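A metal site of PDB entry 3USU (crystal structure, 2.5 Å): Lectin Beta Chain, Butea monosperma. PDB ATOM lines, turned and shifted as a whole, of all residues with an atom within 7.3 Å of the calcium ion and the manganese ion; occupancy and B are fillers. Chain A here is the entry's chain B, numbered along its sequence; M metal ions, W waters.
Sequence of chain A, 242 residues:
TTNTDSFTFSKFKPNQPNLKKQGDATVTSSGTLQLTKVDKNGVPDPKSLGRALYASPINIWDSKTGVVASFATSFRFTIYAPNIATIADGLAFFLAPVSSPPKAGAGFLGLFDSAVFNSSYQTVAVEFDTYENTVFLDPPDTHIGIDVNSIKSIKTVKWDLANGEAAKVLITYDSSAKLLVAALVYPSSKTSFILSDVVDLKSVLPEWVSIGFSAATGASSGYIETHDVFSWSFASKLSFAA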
ATOM      1  N   ASP A  89       5.504   1.835  -1.043  1.00  0.00           N
ATOM      2  CA  ASP A  89       6.088   3.150  -0.844  1.00  0.00           C
ATOM      3  C   ASP A  89       6.246   3.378   0.642  1.00  0.00           C
ATOM      4  O   ASP A  89       7.176   4.065   1.074  1.00  0.00           O
ATOM      5  CB  ASP A  89       5.187   4.251  -1.471  1.00  0.00           C
ATOM      6  CG  ASP A  89       5.751   4.802  -2.747  1.00  0.00           C
ATOM      7  OD1 ASP A  89       6.824   5.435  -2.678  1.00  0.00           O
ATOM      8  OD2 ASP A  89       5.149   4.601  -3.833  1.00  0.00           O
ATOM      9  N   GLY A  90       5.309   2.830   1.408  1.00  0.00           N
ATOM     10  CA  GLY A  90       5.455   2.655   2.835  1.00  0.00           C
ATOM     11  C   GLY A  90       4.122   2.589   3.555  1.00  0.00           C
ATOM     12  O   GLY A  90       3.054   2.523   2.891  1.00  0.00           O
ATOM     13  N   ALA A 106       1.069   6.774  -3.498  1.00  0.00           N
ATOM     14  CA  ALA A 106       2.490   6.548  -3.672  1.00  0.00           C
ATOM     15  C   ALA A 106       3.320   7.071  -2.482  1.00  0.00           C
ATOM     16  O   ALA A 106       2.909   6.887  -1.341  1.00  0.00           O
ATOM     17  CB  ALA A 106       2.937   7.116  -5.037  1.00  0.00           C
ATOM     18  N   GLY A 107       4.438   7.758  -2.752  1.00  0.00           N
ATOM     19  CA  GLY A 107       5.226   8.443  -1.710  1.00  0.00           C
ATOM     20  C   GLY A 107       4.636   9.474  -0.746  1.00  0.00           C
ATOM     21  O   GLY A 107       5.266   9.781   0.253  1.00  0.00           O
ATOM     22  N   PHE A 108       3.456  10.026  -1.022  1.00  0.00           N
ATOM     23  CA  PHE A 108       2.741  10.915  -0.087  1.00  0.00           C
ATOM     24  C   PHE A 108       2.009  10.098   0.997  1.00  0.00           C
ATOM     25  O   PHE A 108       1.507  10.657   1.982  1.00  0.00           O
ATOM     26  CB  PHE A 108       1.683  11.781  -0.812  1.00  0.00           C
ATOM     27  CG  PHE A 108       2.220  12.503  -2.008  1.00  0.00           C
ATOM     28  CD1 PHE A 108       2.788  13.753  -1.888  1.00  0.00           C
ATOM     29  CD2 PHE A 108       2.122  11.936  -3.274  1.00  0.00           C
ATOM     30  CE1 PHE A 108       3.283  14.399  -2.980  1.00  0.00           C
ATOM     31  CE2 PHE A 108       2.597  12.593  -4.388  1.00  0.00           C
ATOM     32  CZ  PHE A 108       3.198  13.825  -4.243  1.00  0.00           C
ATOM     33  N   LEU A 109       1.876   8.791   0.750  1.00  0.00           N
ATOM     34  CA  LEU A 109       1.478   7.822   1.778  1.00  0.00           C
ATOM     35  C   LEU A 109       0.012   7.917   2.220  1.00  0.00           C
ATOM     36  O   LEU A 109      -0.352   7.414   3.282  1.00  0.00           O
ATOM     37  CB  LEU A 109       2.408   7.895   2.987  1.00  0.00           C
ATOM     38  CG  LEU A 109       3.878   7.536   2.830  1.00  0.00           C
ATOM     39  CD1 LEU A 109       4.548   7.639   4.192  1.00  0.00           C
ATOM     40  CD2 LEU A 109       4.056   6.137   2.280  1.00  0.00           C
ATOM     41  N   GLU A 127       6.162   7.402  10.095  1.00  0.00           N
ATOM     42  CA  GLU A 127       6.195   6.729   8.805  1.00  0.00           C
ATOM     43  C   GLU A 127       7.321   5.687   8.738  1.00  0.00           C
ATOM     44  O   GLU A 127       8.361   5.787   9.388  1.00  0.00           O
ATOM     45  CB  GLU A 127       6.367   7.731   7.665  1.00  0.00           C
ATOM     46  CG  GLU A 127       7.760   8.335   7.569  1.00  0.00           C
ATOM     47  CD  GLU A 127       7.958   9.181   6.348  1.00  0.00           C
ATOM     48  OE1 GLU A 127       6.970   9.854   5.956  1.00  0.00           O
ATOM     49  OE2 GLU A 127       9.082   9.207   5.798  1.00  0.00           O
ATOM     50  N   PHE A 128       7.051   4.726   7.859  1.00  0.00           N
ATOM     51  CA  PHE A 128       7.839   3.551   7.679  1.00  0.00           C
ATOM     52  C   PHE A 128       7.987   3.512   6.158  1.00  0.00           C
ATOM     53  O   PHE A 128       7.128   2.935   5.441  1.00  0.00           O
ATOM     54  CB  PHE A 128       7.079   2.335   8.251  1.00  0.00           C
ATOM     55  CG  PHE A 128       6.840   2.417   9.739  1.00  0.00           C
ATOM     56  CD1 PHE A 128       7.836   2.043  10.648  1.00  0.00           C
ATOM     57  CD2 PHE A 128       5.617   2.924  10.244  1.00  0.00           C
ATOM     58  CE1 PHE A 128       7.631   2.165  12.014  1.00  0.00           C
ATOM     59  CE2 PHE A 128       5.415   3.038  11.617  1.00  0.00           C
ATOM     60  CZ  PHE A 128       6.414   2.649  12.511  1.00  0.00           C
ATOM     61  N   ASP A 129       9.058   4.157   5.688  1.00  0.00           N
ATOM     62  CA  ASP A 129       9.194   4.557   4.295  1.00  0.00           C
ATOM     63  C   ASP A 129      10.137   3.661   3.523  1.00  0.00           C
ATOM     64  O   ASP A 129      11.330   3.555   3.838  1.00  0.00           O
ATOM     65  CB  ASP A 129       9.690   6.027   4.220  1.00  0.00           C
ATOM     66  CG  ASP A 129       9.570   6.637   2.788  1.00  0.00           C
ATOM     67  OD1 ASP A 129       9.252   5.943   1.815  1.00  0.00           O
ATOM     68  OD2 ASP A 129       9.815   7.830   2.631  1.00  0.00           O
ATOM     69  N   THR A 130       9.627   3.060   2.463  1.00  0.00           N
ATOM     70  CA  THR A 130      10.430   2.100   1.722  1.00  0.00           C
ATOM     71  C   THR A 130      10.988   2.581   0.387  1.00  0.00           C
ATOM     72  O   THR A 130      11.541   1.775  -0.375  1.00  0.00           O
ATOM     73  CB  THR A 130       9.650   0.815   1.452  1.00  0.00           C
ATOM     74  OG1 THR A 130       8.426   1.155   0.768  1.00  0.00           O
ATOM     75  CG2 THR A 130       9.395   0.100   2.786  1.00  0.00           C
ATOM     76  N   TYR A 131      10.807   3.862   0.085  1.00  0.00           N
ATOM     77  CA  TYR A 131      11.235   4.356  -1.224  1.00  0.00           C
ATOM     78  C   TYR A 131      11.687   5.783  -1.149  1.00  0.00           C
ATOM     79  O   TYR A 131      10.979   6.627  -0.610  1.00  0.00           O
ATOM     80  CB  TYR A 131      10.114   4.206  -2.221  1.00  0.00           C
ATOM     81  CG  TYR A 131      10.427   4.734  -3.591  1.00  0.00           C
ATOM     82  CD1 TYR A 131      11.030   3.910  -4.560  1.00  0.00           C
ATOM     83  CD2 TYR A 131      10.083   6.055  -3.940  1.00  0.00           C
ATOM     84  CE1 TYR A 131      11.289   4.368  -5.828  1.00  0.00           C
ATOM     85  CE2 TYR A 131      10.357   6.529  -5.201  1.00  0.00           C
ATOM     86  CZ  TYR A 131      10.944   5.694  -6.131  1.00  0.00           C
ATOM     87  OH  TYR A 131      11.202   6.176  -7.377  1.00  0.00           O
ATOM     88  N   GLU A 132      12.859   6.044  -1.723  1.00  0.00           N
ATOM     89  CA  GLU A 132      13.459   7.370  -1.705  1.00  0.00           C
ATOM     90  C   GLU A 132      12.789   8.335  -2.694  1.00  0.00           C
ATOM     91  O   GLU A 132      13.051   8.357  -3.915  1.00  0.00           O
ATOM     92  CB  GLU A 132      14.945   7.277  -1.984  1.00  0.00           C
ATOM     93  CG  GLU A 132      15.732   8.434  -1.423  1.00  0.00           C
ATOM     94  CD  GLU A 132      17.175   8.467  -1.924  1.00  0.00           C
ATOM     95  OE1 GLU A 132      17.593   7.576  -2.716  1.00  0.00           O
ATOM     96  OE2 GLU A 132      17.917   9.382  -1.503  1.00  0.00           O
ATOM     97  N   ASN A 133      11.906   9.160  -2.152  1.00  0.00           N
ATOM     98  CA  ASN A 133      11.422  10.291  -2.877  1.00  0.00           C
ATOM     99  C   ASN A 133      12.477  11.356  -2.669  1.00  0.00           C
ATOM    100  O   ASN A 133      12.530  12.015  -1.626  1.00  0.00           O
ATOM    101  CB  ASN A 133      10.069  10.709  -2.366  1.00  0.00           C
ATOM    102  CG  ASN A 133       9.041   9.619  -2.537  1.00  0.00           C
ATOM    103  OD1 ASN A 133       8.421   9.519  -3.594  1.00  0.00           O
ATOM    104  ND2 ASN A 133       8.842   8.790  -1.512  1.00  0.00           N
ATOM    105  N   THR A 134      13.358  11.475  -3.665  1.00  0.00           N
ATOM    106  CA  THR A 134      14.394  12.480  -3.714  1.00  0.00           C
ATOM    107  C   THR A 134      13.802  13.875  -3.523  1.00  0.00           C
ATOM    108  O   THR A 134      14.401  14.729  -2.882  1.00  0.00           O
ATOM    109  CB  THR A 134      15.183  12.391  -5.052  1.00  0.00           C
ATOM    110  OG1 THR A 134      16.445  12.983  -4.878  1.00  0.00           O
ATOM    111  CG2 THR A 134      14.519  13.119  -6.213  1.00  0.00           C
ATOM    112  N   PHE A 136      11.333  14.772  -1.803  1.00  0.00           N
ATOM    113  CA  PHE A 136      10.864  14.949  -0.440  1.00  0.00           C
ATOM    114  C   PHE A 136      12.016  14.986   0.556  1.00  0.00           C
ATOM    115  O   PHE A 136      11.799  14.852   1.784  1.00  0.00           O
ATOM    116  CB  PHE A 136       9.907  13.820  -0.015  1.00  0.00           C
ATOM    117  CG  PHE A 136       8.666  13.681  -0.866  1.00  0.00           C
ATOM    118  CD1 PHE A 136       8.176  14.766  -1.630  1.00  0.00           C
ATOM    119  CD2 PHE A 136       7.971  12.493  -0.904  1.00  0.00           C
ATOM    120  CE1 PHE A 136       7.051  14.643  -2.418  1.00  0.00           C
ATOM    121  CE2 PHE A 136       6.846  12.370  -1.692  1.00  0.00           C
ATOM    122  CZ  PHE A 136       6.386  13.434  -2.459  1.00  0.00           C
ATOM    123  N   LEU A 137      13.219  15.174   0.030  1.00  0.00           N
ATOM    124  CA  LEU A 137      14.462  15.058   0.821  1.00  0.00           C
ATOM    125  C   LEU A 137      14.515  13.762   1.643  1.00  0.00           C
ATOM    126  O   LEU A 137      14.887  13.770   2.784  1.00  0.00           O
ATOM    127  CB  LEU A 137      14.727  16.322   1.678  1.00  0.00           C
ATOM    128  CG  LEU A 137      16.150  16.548   2.272  1.00  0.00           C
ATOM    129  CD1 LEU A 137      17.286  16.138   1.328  1.00  0.00           C
ATOM    130  CD2 LEU A 137      16.439  17.955   2.837  1.00  0.00           C
ATOM    131  N   ASP A 138      14.116  12.645   1.019  1.00  0.00           N
ATOM    132  CA  ASP A 138      14.183  11.283   1.607  1.00  0.00           C
ATOM    133  C   ASP A 138      15.620  10.763   1.771  1.00  0.00           C
ATOM    134  O   ASP A 138      16.398  10.828   0.842  1.00  0.00           O
ATOM    135  CB  ASP A 138      13.423  10.267   0.737  1.00  0.00           C
ATOM    136  CG  ASP A 138      12.029   9.893   1.308  1.00  0.00           C
ATOM    137  OD1 ASP A 138      11.703  10.195   2.521  1.00  0.00           O
ATOM    138  OD2 ASP A 138      11.247   9.290   0.519  1.00  0.00           O
ATOM    139  N   PRO A 139      15.969  10.196   2.932  1.00  0.00           N
ATOM    140  CA  PRO A 139      17.346   9.648   3.040  1.00  0.00           C
ATOM    141  C   PRO A 139      17.601   8.453   2.090  1.00  0.00           C
ATOM    142  O   PRO A 139      16.658   7.849   1.553  1.00  0.00           O
ATOM    143  CB  PRO A 139      17.457   9.232   4.494  1.00  0.00           C
ATOM    144  CG  PRO A 139      16.045   9.017   4.946  1.00  0.00           C
ATOM    145  CD  PRO A 139      15.162   9.931   4.145  1.00  0.00           C
ATOM    146  N   ASP A 141      17.919   5.353   2.132  1.00  0.00           N
ATOM    147  CA  ASP A 141      17.725   4.100   2.819  1.00  0.00           C
ATOM    148  C   ASP A 141      16.284   4.072   3.224  1.00  0.00           C
ATOM    149  O   ASP A 141      15.657   5.112   3.354  1.00  0.00           O
ATOM    150  CB  ASP A 141      18.704   3.944   4.000  1.00  0.00           C
ATOM    151  CG  ASP A 141      18.845   5.209   4.826  1.00  0.00           C
ATOM    152  OD1 ASP A 141      18.232   5.285   5.922  1.00  0.00           O
ATOM    153  OD2 ASP A 141      19.543   6.143   4.368  1.00  0.00           O
ATOM    154  N   HIS A 143      13.602   4.013   5.918  1.00  0.00           N
ATOM    155  CA  HIS A 143      13.757   4.786   7.159  1.00  0.00           C
ATOM    156  C   HIS A 143      12.514   4.801   7.953  1.00  0.00           C
ATOM    157  O   HIS A 143      11.510   4.432   7.442  1.00  0.00           O
ATOM    158  CB  HIS A 143      14.177   6.202   6.844  1.00  0.00           C
ATOM    159  CG  HIS A 143      13.350   6.877   5.763  1.00  0.00           C
ATOM    160  ND1 HIS A 143      13.516   6.604   4.462  1.00  0.00           N
ATOM    161  CD2 HIS A 143      12.390   7.881   5.836  1.00  0.00           C
ATOM    162  CE1 HIS A 143      12.722   7.400   3.742  1.00  0.00           C
ATOM    163  NE2 HIS A 143      12.024   8.166   4.574  1.00  0.00           N
ATOM    164  N   ILE A 144      12.568   5.183   9.228  1.00  0.00           N
ATOM    165  CA  ILE A 144      11.364   5.543   9.975  1.00  0.00           C
ATOM    166  C   ILE A 144      11.437   7.041  10.081  1.00  0.00           C
ATOM    167  O   ILE A 144      12.530   7.571  10.175  1.00  0.00           O
ATOM    168  CB  ILE A 144      11.311   4.984  11.387  1.00  0.00           C
ATOM    169  CG1 ILE A 144      11.295   3.460  11.360  1.00  0.00           C
ATOM    170  CG2 ILE A 144      10.064   5.496  12.105  1.00  0.00           C
ATOM    171  CD1 ILE A 144      11.748   2.801  12.632  1.00  0.00           C
ATOM    172  N   GLY A 145      10.287   7.728  10.011  1.00  0.00           N
ATOM    173  CA  GLY A 145      10.319   9.183  10.053  1.00  0.00           C
ATOM    174  C   GLY A 145       9.204   9.767  10.891  1.00  0.00           C
ATOM    175  O   GLY A 145       8.107   9.211  10.888  1.00  0.00           O
ATOM    176  N   ASP A 147       6.802  12.914  10.826  1.00  0.00           N
ATOM    177  CA  ASP A 147       6.324  13.893   9.850  1.00  0.00           C
ATOM    178  C   ASP A 147       5.258  14.739  10.520  1.00  0.00           C
ATOM    179  O   ASP A 147       4.287  14.221  11.087  1.00  0.00           O
ATOM    180  CB  ASP A 147       5.592  13.235   8.640  1.00  0.00           C
ATOM    181  CG  ASP A 147       6.430  12.210   7.883  1.00  0.00           C
ATOM    182  OD1 ASP A 147       7.649  12.053   8.112  1.00  0.00           O
ATOM    183  OD2 ASP A 147       5.832  11.500   7.046  1.00  0.00           O
ATOM    184  N   ILE A 151       5.372  15.542   4.171  1.00  0.00           N
ATOM    185  CA  ILE A 151       5.957  14.224   3.911  1.00  0.00           C
ATOM    186  C   ILE A 151       7.494  14.302   4.057  1.00  0.00           C
ATOM    187  O   ILE A 151       8.229  13.282   4.095  1.00  0.00           O
ATOM    188  CB  ILE A 151       5.528  13.713   2.516  1.00  0.00           C
ATOM    189  CG1 ILE A 151       6.048  12.279   2.237  1.00  0.00           C
ATOM    190  CG2 ILE A 151       5.884  14.724   1.417  1.00  0.00           C
ATOM    191  CD1 ILE A 151       5.323  11.180   2.982  1.00  0.00           C
ATOM    192  N   LYS A 152       7.970  15.546   4.142  1.00  0.00           N
ATOM    193  CA  LYS A 152       9.352  15.875   4.494  1.00  0.00           C
ATOM    194  C   LYS A 152       9.585  15.661   6.019  1.00  0.00           C
ATOM    195  O   LYS A 152       9.366  16.567   6.837  1.00  0.00           O
ATOM    196  CB  LYS A 152       9.666  17.320   4.067  1.00  0.00           C
ATOM    197  CG  LYS A 152      10.962  17.549   3.284  1.00  0.00           C
ATOM    198  CD  LYS A 152      12.193  17.135   4.083  1.00  0.00           C
ATOM    199  CE  LYS A 152      12.450  18.067   5.253  1.00  0.00           C
ATOM    200  NZ  LYS A 152      13.087  19.333   4.793  1.00  0.00           N
ATOM    201  N   SER A 153       9.998  14.451   6.395  1.00  0.00           N
ATOM    202  CA  SER A 153      10.192  14.117   7.787  1.00  0.00           C
ATOM    203  C   SER A 153      10.989  15.166   8.543  1.00  0.00           C
ATOM    204  O   SER A 153      11.944  15.687   8.015  1.00  0.00           O
ATOM    205  CB  SER A 153      10.859  12.771   7.931  1.00  0.00           C
ATOM    206  OG  SER A 153      10.049  11.773   7.338  1.00  0.00           O
ATOM    207  N   THR A 156      14.634  11.606  10.727  1.00  0.00           N
ATOM    208  CA  THR A 156      14.554  10.180  10.407  1.00  0.00           C
ATOM    209  C   THR A 156      15.624   9.326  11.109  1.00  0.00           C
ATOM    210  O   THR A 156      16.611   9.851  11.626  1.00  0.00           O
ATOM    211  CB  THR A 156      14.635   9.913   8.894  1.00  0.00           C
ATOM    212  OG1 THR A 156      15.877  10.398   8.419  1.00  0.00           O
ATOM    213  CG2 THR A 156      13.455  10.582   8.075  1.00  0.00           C
HETATM  214 CA    CA M   1       9.357   7.837   0.372  1.00  0.00          CA
HETATM  215 MN    MN M   2      10.318   9.294   4.082  1.00  0.00          MN
HETATM  216  O   HOH W   1       7.561   6.693  -0.358  1.00  0.00           O
HETATM  217  O   HOH W   2       8.671  10.643   3.298  1.00  0.00           O
HETATM  218  O   HOH W   3      11.253  11.086   5.287  1.00  0.00           O
HETATM  219  O   HOH W   4       8.075   9.392   1.217  1.00  0.00           O
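The side-chain carboxylate of Glu 127 lies close to the side-chain hydroxyl of Ser 153. O of Asp 141 lies within hydrogen-bond range of ND1 of His 143 (2.8 Å). The backbone NH of Glu 127 lies within hydrogen-bond range of the backbone carbonyl oxygen of Gly 145 (2.8 Å).
Four residues have an atom within 4 Å of the calcium ion: Asp 129, Tyr 131, Asn 133 and Asp 138.
Within 4 Å of the manganese ion: Glu 127, Asp 129, Asp 138 and His 143.
The calcium ion is bound by ND2 of Asn 133 (2.2 Å), water W4 (2.2 Å), O of Tyr 131 (2.2 Å), water W1 (2.3 Å), OD2 of Asp 129 (2.3 Å), OD1 of Asp 129 (2.4 Å) and OD2 of Asp 138 (2.4 Å).
The manganese ion is bound by a ring nitrogen (NE2) of His 143 (2.1 Å), the side-chain carboxylate of Glu 127 (2.1 Å), the side-chain carboxylate of Asp 129 (2.1 Å), water W2 (2.3 Å), the side-chain carboxylate of Asp 138 (2.3 Å) and water W3 (2.4 Å).
Water W2 lies within hydrogen-bond range of O of Ile 151 and OE1 of Glu 127.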
